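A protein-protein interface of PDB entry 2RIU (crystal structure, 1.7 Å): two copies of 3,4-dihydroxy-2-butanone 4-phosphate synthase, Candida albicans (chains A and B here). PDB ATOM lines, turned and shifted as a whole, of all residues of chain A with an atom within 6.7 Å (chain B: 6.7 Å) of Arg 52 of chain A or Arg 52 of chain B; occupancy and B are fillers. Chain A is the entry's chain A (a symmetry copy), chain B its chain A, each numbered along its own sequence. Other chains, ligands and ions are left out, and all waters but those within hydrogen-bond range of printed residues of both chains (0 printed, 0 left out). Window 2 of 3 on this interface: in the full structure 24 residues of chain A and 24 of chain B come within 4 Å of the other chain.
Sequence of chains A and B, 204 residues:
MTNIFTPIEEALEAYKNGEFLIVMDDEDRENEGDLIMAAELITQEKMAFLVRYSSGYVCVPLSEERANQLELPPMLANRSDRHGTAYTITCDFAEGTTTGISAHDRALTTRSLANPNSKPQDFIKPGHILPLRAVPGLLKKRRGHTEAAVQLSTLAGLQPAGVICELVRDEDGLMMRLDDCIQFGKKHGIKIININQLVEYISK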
ATOM      1  N   MET A  47      16.584  -1.677  10.896  1.00  0.00           N
ATOM      2  CA  MET A  47      15.928  -1.028  12.043  1.00  0.00           C
ATOM      3  C   MET A  47      16.298  -1.733  13.344  1.00  0.00           C
ATOM      4  O   MET A  47      16.536  -1.086  14.375  1.00  0.00           O
ATOM      5  CB  MET A  47      14.402  -1.005  11.867  1.00  0.00           C
ATOM      6  CG  MET A  47      13.641  -0.235  12.965  1.00  0.00           C
ATOM      7  SD  MET A  47      14.123   1.498  13.154  1.00  0.00           S
ATOM      8  CE  MET A  47      13.242   2.281  11.810  1.00  0.00           C
ATOM      9  N   ALA A  48      16.347  -3.060  13.300  1.00  0.00           N
ATOM     10  CA  ALA A  48      16.757  -3.830  14.471  1.00  0.00           C
ATOM     11  C   ALA A  48      18.171  -3.426  14.880  1.00  0.00           C
ATOM     12  O   ALA A  48      18.441  -3.237  16.062  1.00  0.00           O
ATOM     13  CB  ALA A  48      16.675  -5.317  14.196  1.00  0.00           C
ATOM     14  N   PHE A  49      19.047  -3.278  13.886  1.00  0.00           N
ATOM     15  CA  PHE A  49      20.429  -2.841  14.094  1.00  0.00           C
ATOM     16  C   PHE A  49      20.483  -1.437  14.707  1.00  0.00           C
ATOM     17  O   PHE A  49      21.176  -1.204  15.706  1.00  0.00           O
ATOM     18  CB  PHE A  49      21.188  -2.881  12.759  1.00  0.00           C
ATOM     19  CG  PHE A  49      22.649  -2.540  12.871  1.00  0.00           C
ATOM     20  CD1 PHE A  49      23.593  -3.533  13.098  1.00  0.00           C
ATOM     21  CD2 PHE A  49      23.082  -1.226  12.731  1.00  0.00           C
ATOM     22  CE1 PHE A  49      24.955  -3.218  13.199  1.00  0.00           C
ATOM     23  CE2 PHE A  49      24.434  -0.905  12.825  1.00  0.00           C
ATOM     24  CZ  PHE A  49      25.369  -1.903  13.062  1.00  0.00           C
ATOM     25  N   LEU A  50      19.738  -0.509  14.113  1.00  0.00           N
ATOM     26  CA  LEU A  50      19.677   0.862  14.608  1.00  0.00           C
ATOM     27  C   LEU A  50      19.230   0.910  16.067  1.00  0.00           C
ATOM     28  O   LEU A  50      19.872   1.544  16.893  1.00  0.00           O
ATOM     29  CB  LEU A  50      18.737   1.704  13.737  1.00  0.00           C
ATOM     30  CG  LEU A  50      18.627   3.187  14.108  1.00  0.00           C
ATOM     31  CD1 LEU A  50      19.998   3.864  14.026  1.00  0.00           C
ATOM     32  CD2 LEU A  50      17.630   3.900  13.209  1.00  0.00           C
ATOM     33  N   VAL A  51      18.130   0.230  16.380  1.00  0.00           N
ATOM     34  CA  VAL A  51      17.619   0.198  17.751  1.00  0.00           C
ATOM     35  C   VAL A  51      18.630  -0.445  18.706  1.00  0.00           C
ATOM     36  O   VAL A  51      18.892   0.080  19.790  1.00  0.00           O
ATOM     37  CB  VAL A  51      16.249  -0.506  17.809  1.00  0.00           C
ATOM     38  CG1 VAL A  51      15.816  -0.773  19.250  1.00  0.00           C
ATOM     39  CG2 VAL A  51      15.212   0.333  17.078  1.00  0.00           C
ATOM     40  N   ARG A  52      19.224  -1.556  18.282  1.00  0.00           N
ATOM     41  CA  ARG A  52      20.171  -2.306  19.115  1.00  0.00           C
ATOM     42  C   ARG A  52      21.329  -1.450  19.641  1.00  0.00           C
ATOM     43  O   ARG A  52      21.742  -1.610  20.795  1.00  0.00           O
ATOM     44  CB  ARG A  52      20.701  -3.519  18.339  1.00  0.00           C
ATOM     45  CG  ARG A  52      21.938  -4.199  18.924  1.00  0.00           C
ATOM     46  CD  ARG A  52      21.683  -4.859  20.280  1.00  0.00           C
ATOM     47  NE  ARG A  52      22.924  -5.438  20.792  1.00  0.00           N
ATOM     48  CZ  ARG A  52      23.822  -4.786  21.529  1.00  0.00           C
ATOM     49  NH1 ARG A  52      23.625  -3.518  21.882  1.00  0.00           N
ATOM     50  NH2 ARG A  52      24.923  -5.415  21.920  1.00  0.00           N
ATOM     51  N   TYR A  53      21.841  -0.547  18.806  1.00  0.00           N
ATOM     52  CA  TYR A  53      23.064   0.193  19.129  1.00  0.00           C
ATOM     53  C   TYR A  53      22.847   1.679  19.416  1.00  0.00           C
ATOM     54  O   TYR A  53      23.806   2.454  19.479  1.00  0.00           O
ATOM     55  CB  TYR A  53      24.082   0.030  17.994  1.00  0.00           C
ATOM     56  CG  TYR A  53      24.555  -1.396  17.849  1.00  0.00           C
ATOM     57  CD1 TYR A  53      24.192  -2.163  16.745  1.00  0.00           C
ATOM     58  CD2 TYR A  53      25.337  -1.989  18.842  1.00  0.00           C
ATOM     59  CE1 TYR A  53      24.625  -3.485  16.624  1.00  0.00           C
ATOM     60  CE2 TYR A  53      25.758  -3.307  18.732  1.00  0.00           C
ATOM     61  CZ  TYR A  53      25.398  -4.044  17.625  1.00  0.00           C
ATOM     62  OH  TYR A  53      25.829  -5.354  17.523  1.00  0.00           O
ATOM     63  N   SER A  54      21.598   2.062  19.619  1.00  0.00           N
ATOM     64  CA  SER A  54      21.254   3.465  19.783  1.00  0.00           C
ATOM     65  C   SER A  54      20.334   3.706  20.979  1.00  0.00           C
ATOM     66  O   SER A  54      19.970   2.772  21.693  1.00  0.00           O
ATOM     67  CB  SER A  54      20.594   3.984  18.508  1.00  0.00           C
ATOM     68  OG  SER A  54      19.241   3.560  18.438  1.00  0.00           O
ATOM     69  N   GLY A  56      17.374   4.360  20.773  1.00  0.00           N
ATOM     70  CA  GLY A  56      16.063   3.816  20.407  1.00  0.00           C
ATOM     71  C   GLY A  56      14.985   4.855  20.169  1.00  0.00           C
ATOM     72  O   GLY A  56      13.869   4.517  19.778  1.00  0.00           O
ATOM     73  N   VAL A 168      24.904   4.597  21.225  1.00  0.00           N
ATOM     74  CA  VAL A 168      25.144   4.487  22.672  1.00  0.00           C
ATOM     75  C   VAL A 168      26.040   3.296  22.999  1.00  0.00           C
ATOM     76  O   VAL A 168      25.956   2.246  22.351  1.00  0.00           O
ATOM     77  CB  VAL A 168      23.831   4.420  23.502  1.00  0.00           C
ATOM     78  CG1 VAL A 168      22.907   5.578  23.163  1.00  0.00           C
ATOM     79  CG2 VAL A 168      23.100   3.115  23.283  1.00  0.00           C
ATOM     80  N   ARG A 169      26.892   3.478  24.004  1.00  0.00           N
ATOM     81  CA  ARG A 169      27.820   2.446  24.452  1.00  0.00           C
ATOM     82  C   ARG A 169      27.097   1.331  25.192  1.00  0.00           C
ATOM     83  O   ARG A 169      26.244   1.603  26.032  1.00  0.00           O
ATOM     84  CB  ARG A 169      28.885   3.058  25.368  1.00  0.00           C
ATOM     85  CG  ARG A 169      29.863   3.971  24.646  1.00  0.00           C
ATOM     86  CD  ARG A 169      30.623   4.867  25.616  1.00  0.00           C
ATOM     87  NE  ARG A 169      31.075   4.136  26.791  1.00  0.00           N
ATOM     88  CZ  ARG A 169      32.210   3.444  26.870  1.00  0.00           C
ATOM     89  NH1 ARG A 169      32.512   2.808  27.995  1.00  0.00           N
ATOM     90  NH2 ARG A 169      33.043   3.381  25.837  1.00  0.00           N
ATOM     91  N   ASP A 170      27.439   0.079  24.879  1.00  0.00           N
ATOM     92  CA  ASP A 170      26.865  -1.083  25.575  1.00  0.00           C
ATOM     93  C   ASP A 170      27.214  -1.112  27.064  1.00  0.00           C
ATOM     94  O   ASP A 170      26.398  -1.523  27.900  1.00  0.00           O
ATOM     95  CB  ASP A 170      27.362  -2.387  24.947  1.00  0.00           C
ATOM     96  CG  ASP A 170      26.584  -2.791  23.706  1.00  0.00           C
ATOM     97  OD1 ASP A 170      25.672  -2.048  23.276  1.00  0.00           O
ATOM     98  OD2 ASP A 170      26.893  -3.878  23.166  1.00  0.00           O
ATOM     99  N   GLU A 171      28.433  -0.685  27.379  1.00  0.00           N
ATOM    100  CA  GLU A 171      28.986  -0.802  28.724  1.00  0.00           C
ATOM    101  C   GLU A 171      28.211  -0.012  29.774  1.00  0.00           C
ATOM    102  O   GLU A 171      27.969  -0.502  30.883  1.00  0.00           O
ATOM    103  CB  GLU A 171      30.448  -0.347  28.730  1.00  0.00           C
ATOM    104  CG  GLU A 171      31.399  -1.259  27.956  1.00  0.00           C
ATOM    105  CD  GLU A 171      31.546  -0.893  26.489  1.00  0.00           C
ATOM    106  OE1 GLU A 171      30.758  -0.065  25.970  1.00  0.00           O
ATOM    107  OE2 GLU A 171      32.469  -1.444  25.848  1.00  0.00           O
ATOM    108  N   GLY A 173      25.845   2.951  28.646  1.00  0.00           N
ATOM    109  CA  GLY A 173      24.775   3.761  28.062  1.00  0.00           C
ATOM    110  C   GLY A 173      25.165   5.188  27.714  1.00  0.00           C
ATOM    111  O   GLY A 173      24.315   5.982  27.325  1.00  0.00           O
ATOM    112  N   MET B  47      18.419   3.575  33.970  1.00  0.00           N
ATOM    113  CA  MET B  47      17.957   4.051  32.656  1.00  0.00           C
ATOM    114  C   MET B  47      18.839   3.496  31.542  1.00  0.00           C
ATOM    115  O   MET B  47      18.346   3.105  30.473  1.00  0.00           O
ATOM    116  CB  MET B  47      17.934   5.587  32.600  1.00  0.00           C
ATOM    117  CG  MET B  47      17.348   6.173  31.301  1.00  0.00           C
ATOM    118  SD  MET B  47      15.653   5.661  30.930  1.00  0.00           S
ATOM    119  CE  MET B  47      14.697   6.727  31.999  1.00  0.00           C
ATOM    120  N   ALA B  48      20.144   3.460  31.789  1.00  0.00           N
ATOM    121  CA  ALA B  48      21.070   2.885  30.818  1.00  0.00           C
ATOM    122  C   ALA B  48      20.706   1.424  30.566  1.00  0.00           C
ATOM    123  O   ALA B  48      20.688   0.981  29.421  1.00  0.00           O
ATOM    124  CB  ALA B  48      22.502   3.013  31.295  1.00  0.00           C
ATOM    125  N   PHE B  49      20.399   0.704  31.645  1.00  0.00           N
ATOM    126  CA  PHE B  49      19.973  -0.696  31.580  1.00  0.00           C
ATOM    127  C   PHE B  49      18.673  -0.846  30.780  1.00  0.00           C
ATOM    128  O   PHE B  49      18.577  -1.680  29.871  1.00  0.00           O
ATOM    129  CB  PHE B  49      19.803  -1.248  33.003  1.00  0.00           C
ATOM    130  CG  PHE B  49      19.456  -2.712  33.058  1.00  0.00           C
ATOM    131  CD1 PHE B  49      20.455  -3.674  33.121  1.00  0.00           C
ATOM    132  CD2 PHE B  49      18.128  -3.125  33.064  1.00  0.00           C
ATOM    133  CE1 PHE B  49      20.134  -5.038  33.176  1.00  0.00           C
ATOM    134  CE2 PHE B  49      17.801  -4.478  33.123  1.00  0.00           C
ATOM    135  CZ  PHE B  49      18.806  -5.433  33.177  1.00  0.00           C
ATOM    136  N   LEU B  50      17.681  -0.025  31.114  1.00  0.00           N
ATOM    137  CA  LEU B  50      16.399  -0.044  30.419  1.00  0.00           C
ATOM    138  C   LEU B  50      16.574   0.182  28.919  1.00  0.00           C
ATOM    139  O   LEU B  50      16.057  -0.579  28.112  1.00  0.00           O
ATOM    140  CB  LEU B  50      15.455   1.010  31.008  1.00  0.00           C
ATOM    141  CG  LEU B  50      14.044   1.058  30.409  1.00  0.00           C
ATOM    142  CD1 LEU B  50      13.339  -0.290  30.591  1.00  0.00           C
ATOM    143  CD2 LEU B  50      13.225   2.174  31.036  1.00  0.00           C
ATOM    144  N   VAL B  51      17.311   1.226  28.552  1.00  0.00           N
ATOM    145  CA  VAL B  51      17.554   1.529  27.141  1.00  0.00           C
ATOM    146  C   VAL B  51      18.312   0.390  26.450  1.00  0.00           C
ATOM    147  O   VAL B  51      17.948  -0.031  25.351  1.00  0.00           O
ATOM    148  CB  VAL B  51      18.283   2.879  26.987  1.00  0.00           C
ATOM    149  CG1 VAL B  51      18.766   3.095  25.554  1.00  0.00           C
ATOM    150  CG2 VAL B  51      17.363   4.008  27.425  1.00  0.00           C
ATOM    151  N   ARG B  52      19.339  -0.129  27.117  1.00  0.00           N
ATOM    152  CA  ARG B  52      20.186  -1.186  26.552  1.00  0.00           C
ATOM    153  C   ARG B  52      19.397  -2.413  26.081  1.00  0.00           C
ATOM    154  O   ARG B  52      19.717  -2.991  25.037  1.00  0.00           O
ATOM    155  CB  ARG B  52      21.263  -1.589  27.568  1.00  0.00           C
ATOM    156  CG  ARG B  52      21.999  -2.897  27.279  1.00  0.00           C
ATOM    157  CD  ARG B  52      22.856  -2.842  26.013  1.00  0.00           C
ATOM    158  NE  ARG B  52      23.482  -4.142  25.780  1.00  0.00           N
ATOM    159  CZ  ARG B  52      22.930  -5.143  25.095  1.00  0.00           C
ATOM    160  NH1 ARG B  52      21.731  -5.006  24.533  1.00  0.00           N
ATOM    161  NH2 ARG B  52      23.590  -6.286  24.968  1.00  0.00           N
ATOM    162  N   TYR B  53      18.372  -2.799  26.839  1.00  0.00           N
ATOM    163  CA  TYR B  53      17.666  -4.060  26.594  1.00  0.00           C
ATOM    164  C   TYR B  53      16.243  -3.895  26.061  1.00  0.00           C
ATOM    165  O   TYR B  53      15.469  -4.856  26.026  1.00  0.00           O
ATOM    166  CB  TYR B  53      17.643  -4.899  27.878  1.00  0.00           C
ATOM    167  CG  TYR B  53      19.023  -5.338  28.300  1.00  0.00           C
ATOM    168  CD1 TYR B  53      19.626  -4.812  29.440  1.00  0.00           C
ATOM    169  CD2 TYR B  53      19.742  -6.256  27.532  1.00  0.00           C
ATOM    170  CE1 TYR B  53      20.908  -5.216  29.818  1.00  0.00           C
ATOM    171  CE2 TYR B  53      21.022  -6.650  27.896  1.00  0.00           C
ATOM    172  CZ  TYR B  53      21.595  -6.127  29.036  1.00  0.00           C
ATOM    173  OH  TYR B  53      22.868  -6.532  29.392  1.00  0.00           O
ATOM    174  N   SER B  54      15.915  -2.691  25.623  1.00  0.00           N
ATOM    175  CA  SER B  54      14.557  -2.381  25.204  1.00  0.00           C
ATOM    176  C   SER B  54      14.511  -1.650  23.864  1.00  0.00           C
ATOM    177  O   SER B  54      15.547  -1.391  23.250  1.00  0.00           O
ATOM    178  CB  SER B  54      13.869  -1.542  26.278  1.00  0.00           C
ATOM    179  OG  SER B  54      14.301  -0.193  26.210  1.00  0.00           O
ATOM    180  N   GLY B  56      13.886   1.306  23.533  1.00  0.00           N
ATOM    181  CA  GLY B  56      14.393   2.658  23.778  1.00  0.00           C
ATOM    182  C   GLY B  56      13.349   3.755  23.699  1.00  0.00           C
ATOM    183  O   GLY B  56      13.646   4.918  23.968  1.00  0.00           O
ATOM    184  N   VAL B 168      13.586  -6.210  24.163  1.00  0.00           N
ATOM    185  CA  VAL B 168      13.904  -6.661  22.799  1.00  0.00           C
ATOM    186  C   VAL B 168      15.114  -7.590  22.787  1.00  0.00           C
ATOM    187  O   VAL B 168      16.059  -7.407  23.564  1.00  0.00           O
ATOM    188  CB  VAL B 168      14.115  -5.484  21.804  1.00  0.00           C
ATOM    189  CG1 VAL B 168      12.936  -4.526  21.829  1.00  0.00           C
ATOM    190  CG2 VAL B 168      15.386  -4.723  22.104  1.00  0.00           C
ATOM    191  N   ARG B 169      15.067  -8.582  21.903  1.00  0.00           N
ATOM    192  CA  ARG B 169      16.137  -9.562  21.754  1.00  0.00           C
ATOM    193  C   ARG B 169      17.362  -8.951  21.089  1.00  0.00           C
ATOM    194  O   ARG B 169      17.231  -8.233  20.102  1.00  0.00           O
ATOM    195  CB  ARG B 169      15.648 -10.753  20.924  1.00  0.00           C
ATOM    196  CG  ARG B 169      14.621 -11.617  21.639  1.00  0.00           C
ATOM    197  CD  ARG B 169      13.865 -12.517  20.669  1.00  0.00           C
ATOM    198  NE  ARG B 169      14.753 -13.135  19.695  1.00  0.00           N
ATOM    199  CZ  ARG B 169      15.429 -14.266  19.887  1.00  0.00           C
ATOM    200  NH1 ARG B 169      16.218 -14.728  18.926  1.00  0.00           N
ATOM    201  NH2 ARG B 169      15.325 -14.936  21.029  1.00  0.00           N
ATOM    202  N   ASP B 170      18.547  -9.238  21.631  1.00  0.00           N
ATOM    203  CA  ASP B 170      19.809  -8.767  21.037  1.00  0.00           C
ATOM    204  C   ASP B 170      20.050  -9.332  19.637  1.00  0.00           C
ATOM    205  O   ASP B 170      20.594  -8.647  18.760  1.00  0.00           O
ATOM    206  CB  ASP B 170      20.998  -9.160  21.918  1.00  0.00           C
ATOM    207  CG  ASP B 170      21.228  -8.205  23.076  1.00  0.00           C
ATOM    208  OD1 ASP B 170      20.447  -7.243  23.253  1.00  0.00           O
ATOM    209  OD2 ASP B 170      22.219  -8.426  23.811  1.00  0.00           O
ATOM    210  N   GLU B 171      19.653 -10.587  19.445  1.00  0.00           N
ATOM    211  CA  GLU B 171      19.957 -11.332  18.228  1.00  0.00           C
ATOM    212  C   GLU B 171      19.343 -10.724  16.970  1.00  0.00           C
ATOM    213  O   GLU B 171      19.996 -10.647  15.922  1.00  0.00           O
ATOM    214  CB  GLU B 171      19.482 -12.781  18.370  1.00  0.00           C
ATOM    215  CG  GLU B 171      20.254 -13.603  19.402  1.00  0.00           C
ATOM    216  CD  GLU B 171      19.674 -13.533  20.803  1.00  0.00           C
ATOM    217  OE1 GLU B 171      18.792 -12.680  21.072  1.00  0.00           O
ATOM    218  OE2 GLU B 171      20.109 -14.349  21.648  1.00  0.00           O
ATOM    219  N   GLY B 173      16.289  -8.232  17.287  1.00  0.00           N
ATOM    220  CA  GLY B 173      15.420  -7.091  17.581  1.00  0.00           C
ATOM    221  C   GLY B 173      13.951  -7.431  17.767  1.00  0.00           C
ATOM    222  O   GLY B 173      13.123  -6.536  17.905  1.00  0.00           O
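The guanidinium group of Arg 52 of chain A lies close to the guanidinium group of Arg 52 of chain B (3.4 Å). NE of Arg 52 of chain B lies within salt-bridge range of OD1 of Asp 170 of chain A (3.9 Å). The guanidinium group of Arg 52 of chain A lies within salt-bridge range of the side-chain carboxylate of Asp 170 of chain B, at 3.9 Å.
Arg 52 of chain A touches its own counterpart, Arg 52 of chain B. Arg 52 of chain A touches Asp 170 of chain B, and with the chains exchanged Asp 170 of chain A touches Arg 52 of chain B. Gly 56 of chain B touches its own counterpart, Gly 56 of chain A. 14 positions are printed for both chains.
The side-chain carboxylate (OD2) of Asp 170 of chain B is in salt-bridge range of the guanidinium group (NH2) of Arg 52 of chain B. OD2 of Asp 170 of chain A is in salt-bridge range of NH2 of Arg 52 of chain A (2.8 Å). The side-chain hydroxyl (OG) of Ser 54 of chain B lies close to the backbone NH (N) of Gly 56 of chain B (3.1 Å). The side-chain hydroxyl of Ser 54 of chain A sits close to the backbone NH of Gly 56 of chain A.
Arg 52 of chain A touches two residues of chain B. Arg 52 of chain B touches just these residues of chain A: Arg 52 and Asp 170. Printed residues of chain A within 4 Å of Gly 56 of chain B: Gly 56. Of the printed residues of chain A, Asp 170 of chain B touches Arg 52. Of the printed residues of chain B, Asp 170 of chain A touches Arg 52. Of the printed residues of chain B, Gly 56 of chain A touches Gly 56. The nearest residue of chain A that does not touch Arg 52 of chain B is Arg 169 of chain A (5.6 Å).
Among the printed residues, pairs that only touch across the chains: Gly 56 of chain A with Gly 56 of chain B.
Of the 14 printed residues of chain B, 3 touch a printed residue of chain A.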
